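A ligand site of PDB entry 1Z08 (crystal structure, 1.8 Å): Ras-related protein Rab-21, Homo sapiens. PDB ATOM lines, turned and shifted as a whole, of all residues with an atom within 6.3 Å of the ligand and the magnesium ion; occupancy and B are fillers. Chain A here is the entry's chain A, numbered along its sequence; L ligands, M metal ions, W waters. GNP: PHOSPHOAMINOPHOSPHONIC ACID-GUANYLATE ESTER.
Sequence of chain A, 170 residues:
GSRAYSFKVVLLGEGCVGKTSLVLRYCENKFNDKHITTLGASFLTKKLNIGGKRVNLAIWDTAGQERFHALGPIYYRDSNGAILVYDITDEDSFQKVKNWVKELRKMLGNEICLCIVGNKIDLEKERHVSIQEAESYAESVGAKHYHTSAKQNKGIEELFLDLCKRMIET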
ATOM      1  N   GLY A  13     -24.203 -19.654 -26.837  1.00  0.00           N
ATOM      2  CA  GLY A  13     -23.997 -19.538 -25.400  1.00  0.00           C
ATOM      3  C   GLY A  13     -24.122 -18.117 -24.884  1.00  0.00           C
ATOM      4  O   GLY A  13     -24.102 -17.161 -25.655  1.00  0.00           O
ATOM      5  N   GLU A  14     -24.233 -17.993 -23.563  1.00  0.00           N
ATOM      6  CA  GLU A  14     -24.420 -16.700 -22.883  1.00  0.00           C
ATOM      7  C   GLU A  14     -23.250 -15.732 -23.076  1.00  0.00           C
ATOM      8  O   GLU A  14     -22.174 -16.113 -23.539  1.00  0.00           O
ATOM      9  CB  GLU A  14     -24.693 -16.924 -21.403  1.00  0.00           C
ATOM     10  CG  GLU A  14     -25.957 -17.725 -21.103  1.00  0.00           C
ATOM     11  CD  GLU A  14     -27.221 -17.005 -21.546  1.00  0.00           C
ATOM     12  OE1 GLU A  14     -27.580 -15.975 -20.923  1.00  0.00           O
ATOM     13  OE2 GLU A  14     -27.854 -17.462 -22.522  1.00  0.00           O
ATOM     14  N   GLY A  15     -23.477 -14.472 -22.697  1.00  0.00           N
ATOM     15  CA  GLY A  15     -22.511 -13.402 -22.940  1.00  0.00           C
ATOM     16  C   GLY A  15     -21.137 -13.513 -22.295  1.00  0.00           C
ATOM     17  O   GLY A  15     -20.185 -12.880 -22.754  1.00  0.00           O
ATOM     18  N   CYS A  16     -21.027 -14.325 -21.243  1.00  0.00           N
ATOM     19  CA  CYS A  16     -19.795 -14.430 -20.464  1.00  0.00           C
ATOM     20  C   CYS A  16     -18.879 -15.588 -20.865  1.00  0.00           C
ATOM     21  O   CYS A  16     -17.752 -15.668 -20.389  1.00  0.00           O
ATOM     22  CB  CYS A  16     -20.117 -14.540 -18.951  1.00  0.00           C
ATOM     23  SG  CYS A  16     -20.604 -16.200 -18.350  1.00  0.00           S
ATOM     24  N   VAL A  17     -19.352 -16.464 -21.753  1.00  0.00           N
ATOM     25  CA  VAL A  17     -18.802 -17.815 -21.852  1.00  0.00           C
ATOM     26  C   VAL A  17     -17.463 -17.983 -22.593  1.00  0.00           C
ATOM     27  O   VAL A  17     -16.668 -18.862 -22.243  1.00  0.00           O
ATOM     28  CB  VAL A  17     -19.856 -18.837 -22.369  1.00  0.00           C
ATOM     29  CG1 VAL A  17     -21.118 -18.758 -21.523  1.00  0.00           C
ATOM     30  CG2 VAL A  17     -20.183 -18.607 -23.833  1.00  0.00           C
ATOM     31  N   GLY A  18     -17.221 -17.151 -23.608  1.00  0.00           N
ATOM     32  CA  GLY A  18     -15.969 -17.199 -24.362  1.00  0.00           C
ATOM     33  C   GLY A  18     -16.071 -17.732 -25.781  1.00  0.00           C
ATOM     34  O   GLY A  18     -15.112 -18.304 -26.295  1.00  0.00           O
ATOM     35  N   LYS A  19     -17.229 -17.541 -26.411  1.00  0.00           N
ATOM     36  CA  LYS A  19     -17.450 -17.986 -27.795  1.00  0.00           C
ATOM     37  C   LYS A  19     -16.410 -17.399 -28.755  1.00  0.00           C
ATOM     38  O   LYS A  19     -15.705 -18.131 -29.450  1.00  0.00           O
ATOM     39  CB  LYS A  19     -18.856 -17.612 -28.279  1.00  0.00           C
ATOM     40  CG  LYS A  19     -20.007 -18.223 -27.479  1.00  0.00           C
ATOM     41  CD  LYS A  19     -21.380 -17.795 -28.022  1.00  0.00           C
ATOM     42  CE  LYS A  19     -21.664 -16.303 -27.847  1.00  0.00           C
ATOM     43  NZ  LYS A  19     -21.597 -15.833 -26.422  1.00  0.00           N
ATOM     44  N   THR A  20     -16.309 -16.065 -28.757  1.00  0.00           N
ATOM     45  CA  THR A  20     -15.366 -15.378 -29.634  1.00  0.00           C
ATOM     46  C   THR A  20     -13.932 -15.774 -29.282  1.00  0.00           C
ATOM     47  O   THR A  20     -13.122 -15.999 -30.180  1.00  0.00           O
ATOM     48  CB  THR A  20     -15.527 -13.846 -29.569  1.00  0.00           C
ATOM     49  OG1 THR A  20     -16.894 -13.499 -29.867  1.00  0.00           O
ATOM     50  CG2 THR A  20     -14.615 -13.138 -30.560  1.00  0.00           C
ATOM     51  N   SER A  21     -13.642 -15.859 -27.987  1.00  0.00           N
ATOM     52  CA  SER A  21     -12.312 -16.263 -27.524  1.00  0.00           C
ATOM     53  C   SER A  21     -11.895 -17.636 -28.053  1.00  0.00           C
ATOM     54  O   SER A  21     -10.738 -17.846 -28.385  1.00  0.00           O
ATOM     55  CB  SER A  21     -12.227 -16.222 -25.998  1.00  0.00           C
ATOM     56  OG  SER A  21     -12.331 -14.883 -25.525  1.00  0.00           O
ATOM     57  N   LEU A  22     -12.847 -18.569 -28.128  1.00  0.00           N
ATOM     58  CA  LEU A  22     -12.565 -19.893 -28.682  1.00  0.00           C
ATOM     59  C   LEU A  22     -12.182 -19.797 -30.157  1.00  0.00           C
ATOM     60  O   LEU A  22     -11.189 -20.385 -30.583  1.00  0.00           O
ATOM     61  CB  LEU A  22     -13.743 -20.853 -28.480  1.00  0.00           C
ATOM     62  CG  LEU A  22     -13.979 -21.381 -27.053  1.00  0.00           C
ATOM     63  CD1 LEU A  22     -15.320 -22.074 -26.949  1.00  0.00           C
ATOM     64  CD2 LEU A  22     -12.872 -22.324 -26.607  1.00  0.00           C
ATOM     65  N   PHE A  31      -5.587 -14.047 -27.818  1.00  0.00           N
ATOM     66  CA  PHE A  31      -6.561 -14.005 -26.719  1.00  0.00           C
ATOM     67  C   PHE A  31      -6.557 -12.637 -26.056  1.00  0.00           C
ATOM     68  O   PHE A  31      -5.511 -12.000 -25.910  1.00  0.00           O
ATOM     69  CB  PHE A  31      -6.278 -15.102 -25.674  1.00  0.00           C
ATOM     70  CG  PHE A  31      -7.199 -15.057 -24.475  1.00  0.00           C
ATOM     71  CD1 PHE A  31      -8.449 -15.666 -24.512  1.00  0.00           C
ATOM     72  CD2 PHE A  31      -6.805 -14.406 -23.308  1.00  0.00           C
ATOM     73  CE1 PHE A  31      -9.303 -15.618 -23.408  1.00  0.00           C
ATOM     74  CE2 PHE A  31      -7.660 -14.351 -22.188  1.00  0.00           C
ATOM     75  CZ  PHE A  31      -8.910 -14.957 -22.239  1.00  0.00           C
ATOM     76  N   ASN A  32      -7.751 -12.200 -25.644  1.00  0.00           N
ATOM     77  CA  ASN A  32      -7.960 -10.942 -24.952  1.00  0.00           C
ATOM     78  C   ASN A  32      -8.712 -11.155 -23.646  1.00  0.00           C
ATOM     79  O   ASN A  32      -9.738 -11.857 -23.623  1.00  0.00           O
ATOM     80  CB  ASN A  32      -8.761  -9.979 -25.821  1.00  0.00           C
ATOM     81  CG  ASN A  32      -8.055  -9.647 -27.121  1.00  0.00           C
ATOM     82  OD1 ASN A  32      -6.887  -9.260 -27.117  1.00  0.00           O
ATOM     83  ND2 ASN A  32      -8.761  -9.803 -28.237  1.00  0.00           N
ATOM     84  N   ASP A  33      -8.216 -10.564 -22.561  1.00  0.00           N
ATOM     85  CA  ASP A  33      -8.936 -10.554 -21.286  1.00  0.00           C
ATOM     86  C   ASP A  33     -10.160  -9.644 -21.351  1.00  0.00           C
ATOM     87  O   ASP A  33     -11.102  -9.799 -20.574  1.00  0.00           O
ATOM     88  CB  ASP A  33      -8.030 -10.131 -20.124  1.00  0.00           C
ATOM     89  CG  ASP A  33      -7.245 -11.286 -19.521  1.00  0.00           C
ATOM     90  OD1 ASP A  33      -7.774 -12.415 -19.430  1.00  0.00           O
ATOM     91  OD2 ASP A  33      -6.083 -11.060 -19.131  1.00  0.00           O
ATOM     92  N   LYS A  34     -10.123  -8.686 -22.280  1.00  0.00           N
ATOM     93  CA  LYS A  34     -11.252  -7.779 -22.503  1.00  0.00           C
ATOM     94  C   LYS A  34     -12.416  -8.528 -23.134  1.00  0.00           C
ATOM     95  O   LYS A  34     -12.228  -9.371 -24.017  1.00  0.00           O
ATOM     96  CB  LYS A  34     -10.840  -6.603 -23.408  1.00  0.00           C
ATOM     97  CG  LYS A  34     -11.913  -5.519 -23.531  1.00  0.00           C
ATOM     98  CD  LYS A  34     -11.493  -4.422 -24.496  1.00  0.00           C
ATOM     99  CE  LYS A  34     -12.621  -3.409 -24.690  1.00  0.00           C
ATOM    100  NZ  LYS A  34     -12.232  -2.280 -25.570  1.00  0.00           N
ATOM    101  N   HIS A  35     -13.619  -8.228 -22.656  1.00  0.00           N
ATOM    102  CA  HIS A  35     -14.849  -8.728 -23.270  1.00  0.00           C
ATOM    103  C   HIS A  35     -15.231  -7.779 -24.415  1.00  0.00           C
ATOM    104  O   HIS A  35     -15.854  -6.732 -24.198  1.00  0.00           O
ATOM    105  CB  HIS A  35     -15.948  -8.867 -22.215  1.00  0.00           C
ATOM    106  CG  HIS A  35     -17.320  -9.101 -22.772  1.00  0.00           C
ATOM    107  ND1 HIS A  35     -17.577 -10.052 -23.735  1.00  0.00           N
ATOM    108  CD2 HIS A  35     -18.504  -8.512 -22.501  1.00  0.00           C
ATOM    109  CE1 HIS A  35     -18.862 -10.037 -24.036  1.00  0.00           C
ATOM    110  NE2 HIS A  35     -19.449  -9.112 -23.305  1.00  0.00           N
ATOM    111  N   ILE A  36     -14.798  -8.134 -25.623  1.00  0.00           N
ATOM    112  CA  ILE A  36     -15.127  -7.347 -26.810  1.00  0.00           C
ATOM    113  C   ILE A  36     -16.440  -7.883 -27.374  1.00  0.00           C
ATOM    114  O   ILE A  36     -16.462  -8.799 -28.199  1.00  0.00           O
ATOM    115  CB  ILE A  36     -13.994  -7.379 -27.869  1.00  0.00           C
ATOM    116  CG1 ILE A  36     -12.648  -7.053 -27.223  1.00  0.00           C
ATOM    117  CG2 ILE A  36     -14.291  -6.396 -29.013  1.00  0.00           C
ATOM    118  CD1 ILE A  36     -11.427  -7.411 -28.066  1.00  0.00           C
ATOM    119  N   THR A  37     -17.531  -7.292 -26.891  1.00  0.00           N
ATOM    120  CA  THR A  37     -18.885  -7.759 -27.147  1.00  0.00           C
ATOM    121  C   THR A  37     -19.189  -7.953 -28.631  1.00  0.00           C
ATOM    122  O   THR A  37     -18.970  -7.050 -29.445  1.00  0.00           O
ATOM    123  CB  THR A  37     -19.924  -6.784 -26.528  1.00  0.00           C
ATOM    124  OG1 THR A  37     -19.501  -6.441 -25.197  1.00  0.00           O
ATOM    125  CG2 THR A  37     -21.312  -7.410 -26.465  1.00  0.00           C
ATOM    126  N   THR A  38     -19.681  -9.137 -28.962  1.00  0.00           N
ATOM    127  CA  THR A  38     -20.122  -9.454 -30.325  1.00  0.00           C
ATOM    128  C   THR A  38     -21.527  -8.895 -30.517  1.00  0.00           C
ATOM    129  O   THR A  38     -22.436  -9.202 -29.740  1.00  0.00           O
ATOM    130  CB  THR A  38     -20.106 -10.965 -30.581  1.00  0.00           C
ATOM    131  OG1 THR A  38     -18.798 -11.491 -30.276  1.00  0.00           O
ATOM    132  CG2 THR A  38     -20.446 -11.290 -32.031  1.00  0.00           C
ATOM    133  N   LEU A  39     -21.689  -8.079 -31.553  1.00  0.00           N
ATOM    134  CA  LEU A  39     -22.932  -7.350 -31.788  1.00  0.00           C
ATOM    135  C   LEU A  39     -23.886  -8.052 -32.744  1.00  0.00           C
ATOM    136  O   LEU A  39     -25.069  -7.698 -32.827  1.00  0.00           O
ATOM    137  CB  LEU A  39     -22.609  -5.940 -32.304  1.00  0.00           C
ATOM    138  CG  LEU A  39     -21.716  -5.061 -31.426  1.00  0.00           C
ATOM    139  CD1 LEU A  39     -21.392  -3.754 -32.145  1.00  0.00           C
ATOM    140  CD2 LEU A  39     -22.362  -4.779 -30.065  1.00  0.00           C
ATOM    141  N   ASP A  61     -19.909 -17.228 -35.352  1.00  0.00           N
ATOM    142  CA  ASP A  61     -19.957 -16.633 -34.020  1.00  0.00           C
ATOM    143  C   ASP A  61     -21.281 -15.881 -33.882  1.00  0.00           C
ATOM    144  O   ASP A  61     -21.813 -15.378 -34.880  1.00  0.00           O
ATOM    145  CB  ASP A  61     -18.788 -15.668 -33.845  1.00  0.00           C
ATOM    146  CG  ASP A  61     -18.463 -15.366 -32.387  1.00  0.00           C
ATOM    147  OD1 ASP A  61     -19.152 -15.884 -31.473  1.00  0.00           O
ATOM    148  OD2 ASP A  61     -17.500 -14.618 -32.153  1.00  0.00           O
ATOM    149  N   THR A  62     -21.813 -15.810 -32.662  1.00  0.00           N
ATOM    150  CA  THR A  62     -23.104 -15.151 -32.409  1.00  0.00           C
ATOM    151  C   THR A  62     -23.046 -14.146 -31.258  1.00  0.00           C
ATOM    152  O   THR A  62     -22.140 -14.196 -30.434  1.00  0.00           O
ATOM    153  CB  THR A  62     -24.223 -16.177 -32.070  1.00  0.00           C
ATOM    154  OG1 THR A  62     -23.777 -17.063 -31.022  1.00  0.00           O
ATOM    155  CG2 THR A  62     -24.621 -17.002 -33.289  1.00  0.00           C
ATOM    156  N   ALA A  63     -24.017 -13.244 -31.221  1.00  0.00           N
ATOM    157  CA  ALA A  63     -24.196 -12.340 -30.084  1.00  0.00           C
ATOM    158  C   ALA A  63     -24.891 -13.104 -28.968  1.00  0.00           C
ATOM    159  O   ALA A  63     -26.036 -13.541 -29.118  1.00  0.00           O
ATOM    160  CB  ALA A  63     -25.009 -11.123 -30.496  1.00  0.00           C
ATOM    161  N   GLY A  64     -24.205 -13.279 -27.836  1.00  0.00           N
ATOM    162  CA  GLY A  64     -24.714 -14.063 -26.721  1.00  0.00           C
ATOM    163  C   GLY A  64     -25.735 -13.342 -25.856  1.00  0.00           C
ATOM    164  O   GLY A  64     -26.438 -13.971 -25.053  1.00  0.00           O
ATOM    165  N   GLN A  65     -25.803 -12.027 -26.008  1.00  0.00           N
ATOM    166  CA  GLN A  65     -26.744 -11.197 -25.258  1.00  0.00           C
ATOM    167  C   GLN A  65     -27.990 -10.896 -26.098  1.00  0.00           C
ATOM    168  O   GLN A  65     -28.494 -11.754 -26.826  1.00  0.00           O
ATOM    169  CB  GLN A  65     -26.076  -9.905 -24.808  1.00  0.00           C
ATOM    170  N   ASP A  87     -19.566 -21.397 -19.212  1.00  0.00           N
ATOM    171  CA  ASP A  87     -18.487 -20.955 -18.349  1.00  0.00           C
ATOM    172  C   ASP A  87     -18.522 -21.853 -17.110  1.00  0.00           C
ATOM    173  O   ASP A  87     -19.543 -21.923 -16.425  1.00  0.00           O
ATOM    174  CB  ASP A  87     -18.769 -19.481 -17.981  1.00  0.00           C
ATOM    175  CG  ASP A  87     -17.715 -18.866 -17.070  1.00  0.00           C
ATOM    176  OD1 ASP A  87     -17.657 -17.623 -17.038  1.00  0.00           O
ATOM    177  OD2 ASP A  87     -16.975 -19.593 -16.375  1.00  0.00           O
ATOM    178  N   ASN A 119     -15.945 -24.179 -20.890  1.00  0.00           N
ATOM    179  CA  ASN A 119     -14.805 -23.298 -21.112  1.00  0.00           C
ATOM    180  C   ASN A 119     -14.316 -22.646 -19.826  1.00  0.00           C
ATOM    181  O   ASN A 119     -15.038 -22.589 -18.831  1.00  0.00           O
ATOM    182  CB  ASN A 119     -15.141 -22.241 -22.171  1.00  0.00           C
ATOM    183  CG  ASN A 119     -13.928 -21.428 -22.596  1.00  0.00           C
ATOM    184  OD1 ASN A 119     -12.847 -21.974 -22.853  1.00  0.00           O
ATOM    185  ND2 ASN A 119     -14.103 -20.113 -22.673  1.00  0.00           N
ATOM    186  N   LYS A 120     -13.074 -22.152 -19.880  1.00  0.00           N
ATOM    187  CA  LYS A 120     -12.407 -21.468 -18.752  1.00  0.00           C
ATOM    188  C   LYS A 120     -11.887 -22.452 -17.703  1.00  0.00           C
ATOM    189  O   LYS A 120     -11.897 -22.155 -16.503  1.00  0.00           O
ATOM    190  CB  LYS A 120     -13.302 -20.399 -18.107  1.00  0.00           C
ATOM    191  CG  LYS A 120     -13.869 -19.354 -19.067  1.00  0.00           C
ATOM    192  CD  LYS A 120     -14.439 -18.169 -18.309  1.00  0.00           C
ATOM    193  CE  LYS A 120     -15.169 -17.230 -19.242  1.00  0.00           C
ATOM    194  NZ  LYS A 120     -15.736 -16.061 -18.501  1.00  0.00           N
ATOM    195  N   ILE A 121     -11.407 -23.624 -18.148  1.00  0.00           N
ATOM    196  CA  ILE A 121     -10.889 -24.627 -17.205  1.00  0.00           C
ATOM    197  C   ILE A 121      -9.627 -24.171 -16.467  1.00  0.00           C
ATOM    198  O   ILE A 121      -9.235 -24.775 -15.460  1.00  0.00           O
ATOM    199  CB  ILE A 121     -10.687 -26.039 -17.851  1.00  0.00           C
ATOM    200  CG1 ILE A 121      -9.642 -25.980 -18.979  1.00  0.00           C
ATOM    201  CG2 ILE A 121     -12.039 -26.620 -18.297  1.00  0.00           C
ATOM    202  CD1 ILE A 121      -9.232 -27.351 -19.516  1.00  0.00           C
ATOM    203  N   ASP A 122      -9.021 -23.092 -16.946  1.00  0.00           N
ATOM    204  CA  ASP A 122      -7.912 -22.444 -16.233  1.00  0.00           C
ATOM    205  C   ASP A 122      -8.394 -21.818 -14.915  1.00  0.00           C
ATOM    206  O   ASP A 122      -7.590 -21.517 -14.028  1.00  0.00           O
ATOM    207  CB  ASP A 122      -7.242 -21.390 -17.124  1.00  0.00           C
ATOM    208  CG  ASP A 122      -8.196 -20.303 -17.583  1.00  0.00           C
ATOM    209  OD1 ASP A 122      -9.069 -20.586 -18.422  1.00  0.00           O
ATOM    210  OD2 ASP A 122      -8.075 -19.160 -17.094  1.00  0.00           O
ATOM    211  N   LEU A 123      -9.713 -21.645 -14.794  1.00  0.00           N
ATOM    212  CA  LEU A 123     -10.342 -21.125 -13.593  1.00  0.00           C
ATOM    213  C   LEU A 123     -10.982 -22.247 -12.764  1.00  0.00           C
ATOM    214  O   LEU A 123     -12.021 -22.052 -12.126  1.00  0.00           O
ATOM    215  CB  LEU A 123     -11.385 -20.055 -13.941  1.00  0.00           C
ATOM    216  CG  LEU A 123     -10.930 -18.819 -14.728  1.00  0.00           C
ATOM    217  CD1 LEU A 123     -12.125 -17.906 -15.000  1.00  0.00           C
ATOM    218  CD2 LEU A 123      -9.834 -18.053 -13.999  1.00  0.00           C
ATOM    219  N   THR A 148     -12.418 -26.866 -22.303  1.00  0.00           N
ATOM    220  CA  THR A 148     -11.510 -25.945 -22.981  1.00  0.00           C
ATOM    221  C   THR A 148     -11.044 -24.791 -22.108  1.00  0.00           C
ATOM    222  O   THR A 148     -11.689 -24.444 -21.118  1.00  0.00           O
ATOM    223  CB  THR A 148     -12.162 -25.304 -24.237  1.00  0.00           C
ATOM    224  OG1 THR A 148     -13.334 -24.575 -23.849  1.00  0.00           O
ATOM    225  CG2 THR A 148     -12.520 -26.355 -25.289  1.00  0.00           C
ATOM    226  N   SER A 149      -9.907 -24.217 -22.482  1.00  0.00           N
ATOM    227  CA  SER A 149      -9.469 -22.899 -22.019  1.00  0.00           C
ATOM    228  C   SER A 149      -8.950 -22.126 -23.223  1.00  0.00           C
ATOM    229  O   SER A 149      -7.895 -22.449 -23.777  1.00  0.00           O
ATOM    230  CB  SER A 149      -8.380 -23.009 -20.952  1.00  0.00           C
ATOM    231  OG  SER A 149      -7.863 -21.720 -20.626  1.00  0.00           O
ATOM    232  N   ALA A 150      -9.694 -21.100 -23.632  1.00  0.00           N
ATOM    233  CA  ALA A 150      -9.252 -20.199 -24.685  1.00  0.00           C
ATOM    234  C   ALA A 150      -8.020 -19.409 -24.236  1.00  0.00           C
ATOM    235  O   ALA A 150      -7.123 -19.128 -25.035  1.00  0.00           O
ATOM    236  CB  ALA A 150     -10.375 -19.262 -25.105  1.00  0.00           C
ATOM    237  N   LYS A 151      -7.978 -19.077 -22.944  1.00  0.00           N
ATOM    238  CA  LYS A 151      -6.859 -18.310 -22.365  1.00  0.00           C
ATOM    239  C   LYS A 151      -5.531 -19.061 -22.402  1.00  0.00           C
ATOM    240  O   LYS A 151      -4.491 -18.480 -22.732  1.00  0.00           O
ATOM    241  CB  LYS A 151      -7.197 -17.863 -20.932  1.00  0.00           C
ATOM    242  CG  LYS A 151      -6.125 -16.992 -20.271  1.00  0.00           C
ATOM    243  CD  LYS A 151      -6.668 -16.209 -19.086  1.00  0.00           C
ATOM    244  CE  LYS A 151      -5.628 -15.239 -18.566  1.00  0.00           C
ATOM    245  NZ  LYS A 151      -6.235 -14.136 -17.763  1.00  0.00           N
ATOM    246  N   GLN A 152      -5.568 -20.358 -22.066  1.00  0.00           N
ATOM    247  CA  GLN A 152      -4.355 -21.186 -22.058  1.00  0.00           C
ATOM    248  C   GLN A 152      -4.186 -22.056 -23.311  1.00  0.00           C
ATOM    249  O   GLN A 152      -3.228 -22.825 -23.409  1.00  0.00           O
ATOM    250  CB  GLN A 152      -4.328 -22.073 -20.804  1.00  0.00           C
ATOM    251  CG  GLN A 152      -4.265 -21.294 -19.496  1.00  0.00           C
ATOM    252  CD  GLN A 152      -4.143 -22.182 -18.269  1.00  0.00           C
ATOM    253  OE1 GLN A 152      -4.651 -23.306 -18.248  1.00  0.00           O
ATOM    254  NE2 GLN A 152      -3.466 -21.681 -17.244  1.00  0.00           N
HETATM  255  PG  GNP L   1     -20.445 -12.212 -26.398  1.00  0.00           P
HETATM  256  O1G GNP L   1     -21.049 -11.049 -25.640  1.00  0.00           O
HETATM  257  O2G GNP L   1     -19.650 -11.821 -27.618  1.00  0.00           O
HETATM  258  O3G GNP L   1     -21.615 -13.123 -26.641  1.00  0.00           O
HETATM  259  N3B GNP L   1     -19.426 -12.983 -25.416  1.00  0.00           N
HETATM  260  PB  GNP L   1     -18.422 -14.178 -25.765  1.00  0.00           P
HETATM  261  O1B GNP L   1     -19.030 -15.484 -25.479  1.00  0.00           O
HETATM  262  O2B GNP L   1     -17.910 -13.982 -27.148  1.00  0.00           O
HETATM  263  O3A GNP L   1     -17.230 -14.090 -24.791  1.00  0.00           O
HETATM  264  PA  GNP L   1     -15.824 -13.511 -25.022  1.00  0.00           P
HETATM  265  O1A GNP L   1     -15.034 -14.434 -25.857  1.00  0.00           O
HETATM  266  O2A GNP L   1     -15.860 -12.088 -25.447  1.00  0.00           O
HETATM  267  O5' GNP L   1     -15.164 -13.553 -23.596  1.00  0.00           O
HETATM  268  C5' GNP L   1     -15.837 -12.999 -22.471  1.00  0.00           C
HETATM  269  C4' GNP L   1     -14.887 -12.894 -21.292  1.00  0.00           C
HETATM  270  O4' GNP L   1     -14.447 -14.211 -20.886  1.00  0.00           O
HETATM  271  C3' GNP L   1     -13.618 -12.087 -21.568  1.00  0.00           C
HETATM  272  O3' GNP L   1     -13.290 -11.368 -20.400  1.00  0.00           O
HETATM  273  C2' GNP L   1     -12.598 -13.185 -21.888  1.00  0.00           C
HETATM  274  O2' GNP L   1     -11.252 -12.823 -21.669  1.00  0.00           O
HETATM  275  C1' GNP L   1     -13.041 -14.275 -20.917  1.00  0.00           C
HETATM  276  N9  GNP L   1     -12.617 -15.613 -21.316  1.00  0.00           N
HETATM  277  C8  GNP L   1     -12.911 -16.277 -22.491  1.00  0.00           C
HETATM  278  N7  GNP L   1     -12.384 -17.463 -22.557  1.00  0.00           N
HETATM  279  C5  GNP L   1     -11.698 -17.611 -21.354  1.00  0.00           C
HETATM  280  C6  GNP L   1     -10.936 -18.688 -20.839  1.00  0.00           C
HETATM  281  O6  GNP L   1     -10.704 -19.782 -21.379  1.00  0.00           O
HETATM  282  N1  GNP L   1     -10.419 -18.429 -19.574  1.00  0.00           N
HETATM  283  C2  GNP L   1     -10.618 -17.263 -18.878  1.00  0.00           C
HETATM  284  N2  GNP L   1     -10.041 -17.173 -17.665  1.00  0.00           N
HETATM  285  N3  GNP L   1     -11.335 -16.246 -19.337  1.00  0.00           N
HETATM  286  C4  GNP L   1     -11.841 -16.478 -20.580  1.00  0.00           C
HETATM  287 MG    MG M   1     -18.287 -12.759 -28.634  1.00  0.00          MG
HETATM  288  O   HOH W   1     -10.319 -12.695 -18.803  1.00  0.00           O
HETATM  289  O   HOH W   2     -19.675 -14.081 -29.471  1.00  0.00           O
HETATM  290  O   HOH W   3     -13.790 -12.266 -17.878  1.00  0.00           O
HETATM  291  O   HOH W   4     -23.277 -10.290 -27.174  1.00  0.00           O
HETATM  292  O   HOH W   5     -13.400 -10.649 -26.014  1.00  0.00           O
HETATM  293  O   HOH W   6     -22.852 -10.198 -23.705  1.00  0.00           O
HETATM  294  O   HOH W   7     -13.258 -14.849 -17.503  1.00  0.00           O
HETATM  295  O   HOH W   8     -16.901 -11.457 -27.903  1.00  0.00           O
HETATM  296  O   HOH W   9     -10.121 -14.480 -16.509  1.00  0.00           O
HETATM  297  O   HOH W  10     -14.789  -9.917 -18.623  1.00  0.00           O
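O2B of the ligand sits close to N of Thr 20 (3.1 Å).
The backbone NH (N) of Thr 38 sits close to an oxygen (O2G) of the ligand (3.0 Å).
The backbone carbonyl oxygen of Asn 32 lies within hydrogen-bond range of an oxygen (O2') of the ligand, 2.7 Å away.
O of Asp 33 sits at hydrogen-bond distance from O3' of the ligand (2.7 Å).
An oxygen (O1B) of the ligand is in hydrogen-bond range of the backbone NH (N) of Lys 19 (2.9 Å).
The side-chain amino group (NZ) of Lys 19 lies within salt-bridge range of an oxygen (O3G) of the ligand (2.7 Å).
N of Ser 21 is in hydrogen-bond range of O1A of the ligand, at 2.9 Å.
An oxygen (O1A) of the ligand sits at hydrogen-bond distance from the side-chain hydroxyl (OG) of Ser 21, 2.8 Å away.
N3B of the ligand lies within hydrogen-bond range of O of Gly 15 (2.8 Å).
The side-chain carboxylate (OD1) of Asp 122 lies within hydrogen-bond range of a nitrogen (N1) of the ligand, 2.8 Å away.
N of Ala 150 lies within hydrogen-bond range of O6 of the ligand (2.8 Å).
The backbone NH (N) of Gly 64 lies within hydrogen-bond range of an oxygen (O3G) of the ligand (2.9 Å).
A ring nitrogen (ND1) of His 35 lies within hydrogen-bond range of an oxygen (O2A) of the ligand, at 3.2 Å.
N of Gly 18 sits at hydrogen-bond distance from O1B of the ligand (3.1 Å).
The side-chain amide nitrogen (ND2) of Asn 119 is in hydrogen-bond range of a nitrogen (N7) of the ligand (3.2 Å).
N of Lys 151 lies within hydrogen-bond range of O6 of the ligand, at 3.2 Å.
An oxygen (O4') of the ligand is in hydrogen-bond range of the side-chain amino group of Lys 120, 3.3 Å away.
The side-chain carboxylate (OD1) of Asp 33 is in salt-bridge range of the side-chain amino group (NZ) of Lys 151.
O of Glu 14 is in hydrogen-bond range of NZ of Lys 19.
OG of Ser 149 lies within hydrogen-bond range of OD1 of Asp 122 (2.8 Å).
O of Val 17 sits at hydrogen-bond distance from ND2 of Asn 119 (2.9 Å).
The side-chain amide oxygen (OD1) of Asn 119 sits at hydrogen-bond distance from the side-chain hydroxyl (OG1) of Thr 148 (2.8 Å).
The side-chain amino group (NZ) of Lys 120 lies within salt-bridge range of the side-chain carboxylate (OD1) of Asp 87.
N of Gln 152 sits at hydrogen-bond distance from OG of Ser 149 (3.0 Å).
SG of Cys 16 is in hydrogen-bond range of OD1 of Asp 87.
Residues that only touch the ligand: Phe 31 (3.2 Å), Ser 149 (3.4 Å), Leu 123 (3.5 Å), Cys 16 (3.6 Å), Val 17 (3.7 Å), Thr 37 (3.7 Å), Glu 14 (3.7 Å), Lys 34 (3.9 Å) and Thr 62 (3.98 Å).
The nearest printed residue that does not touch the ligand is Ala 63 (4.02 Å).
Within 4 Å of the magnesium ion: Thr 20 and Thr 38.
Along chain A the residues within 4 Å of the magnesium ion span positions 20 to 38.
The nearest printed residue that does not touch the magnesium ion is Asp 61 (4.1 Å).
The magnesium ion is bound by O2G of the ligand (1.9 Å), O2B of the ligand (2.0 Å), OG1 of Thr 20 (2.0 Å), water W8 (2.0 Å), water W2 (2.1 Å) and OG1 of Thr 38 (2.1 Å).
Water W2 bridges O of Thr 62 (2.6 Å) and OD1 of Asp 61 (2.7 Å).
Water W8 lies within hydrogen-bond range of the backbone carbonyl oxygen of Ile 36 (2.7 Å) and an oxygen (O2A) of the ligand (2.7 Å).
Water W4 lies within hydrogen-bond range of O1G of the ligand (2.8 Å), O of Thr 38 (2.9 Å), N of Gly 64 (3.2 Å) and N of Gln 65 (3.3 Å).
Water W5 lies within hydrogen-bond range of the backbone carbonyl oxygen of Lys 34, the backbone NH of Ile 36 and an oxygen (O2A) of the ligand.
Water W7 bridges NZ of Lys 120 and N3 of the ligand.
Water W1 bridges the side-chain carboxylate (OD1) of Asp 33 and an oxygen (O2') of the ligand.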
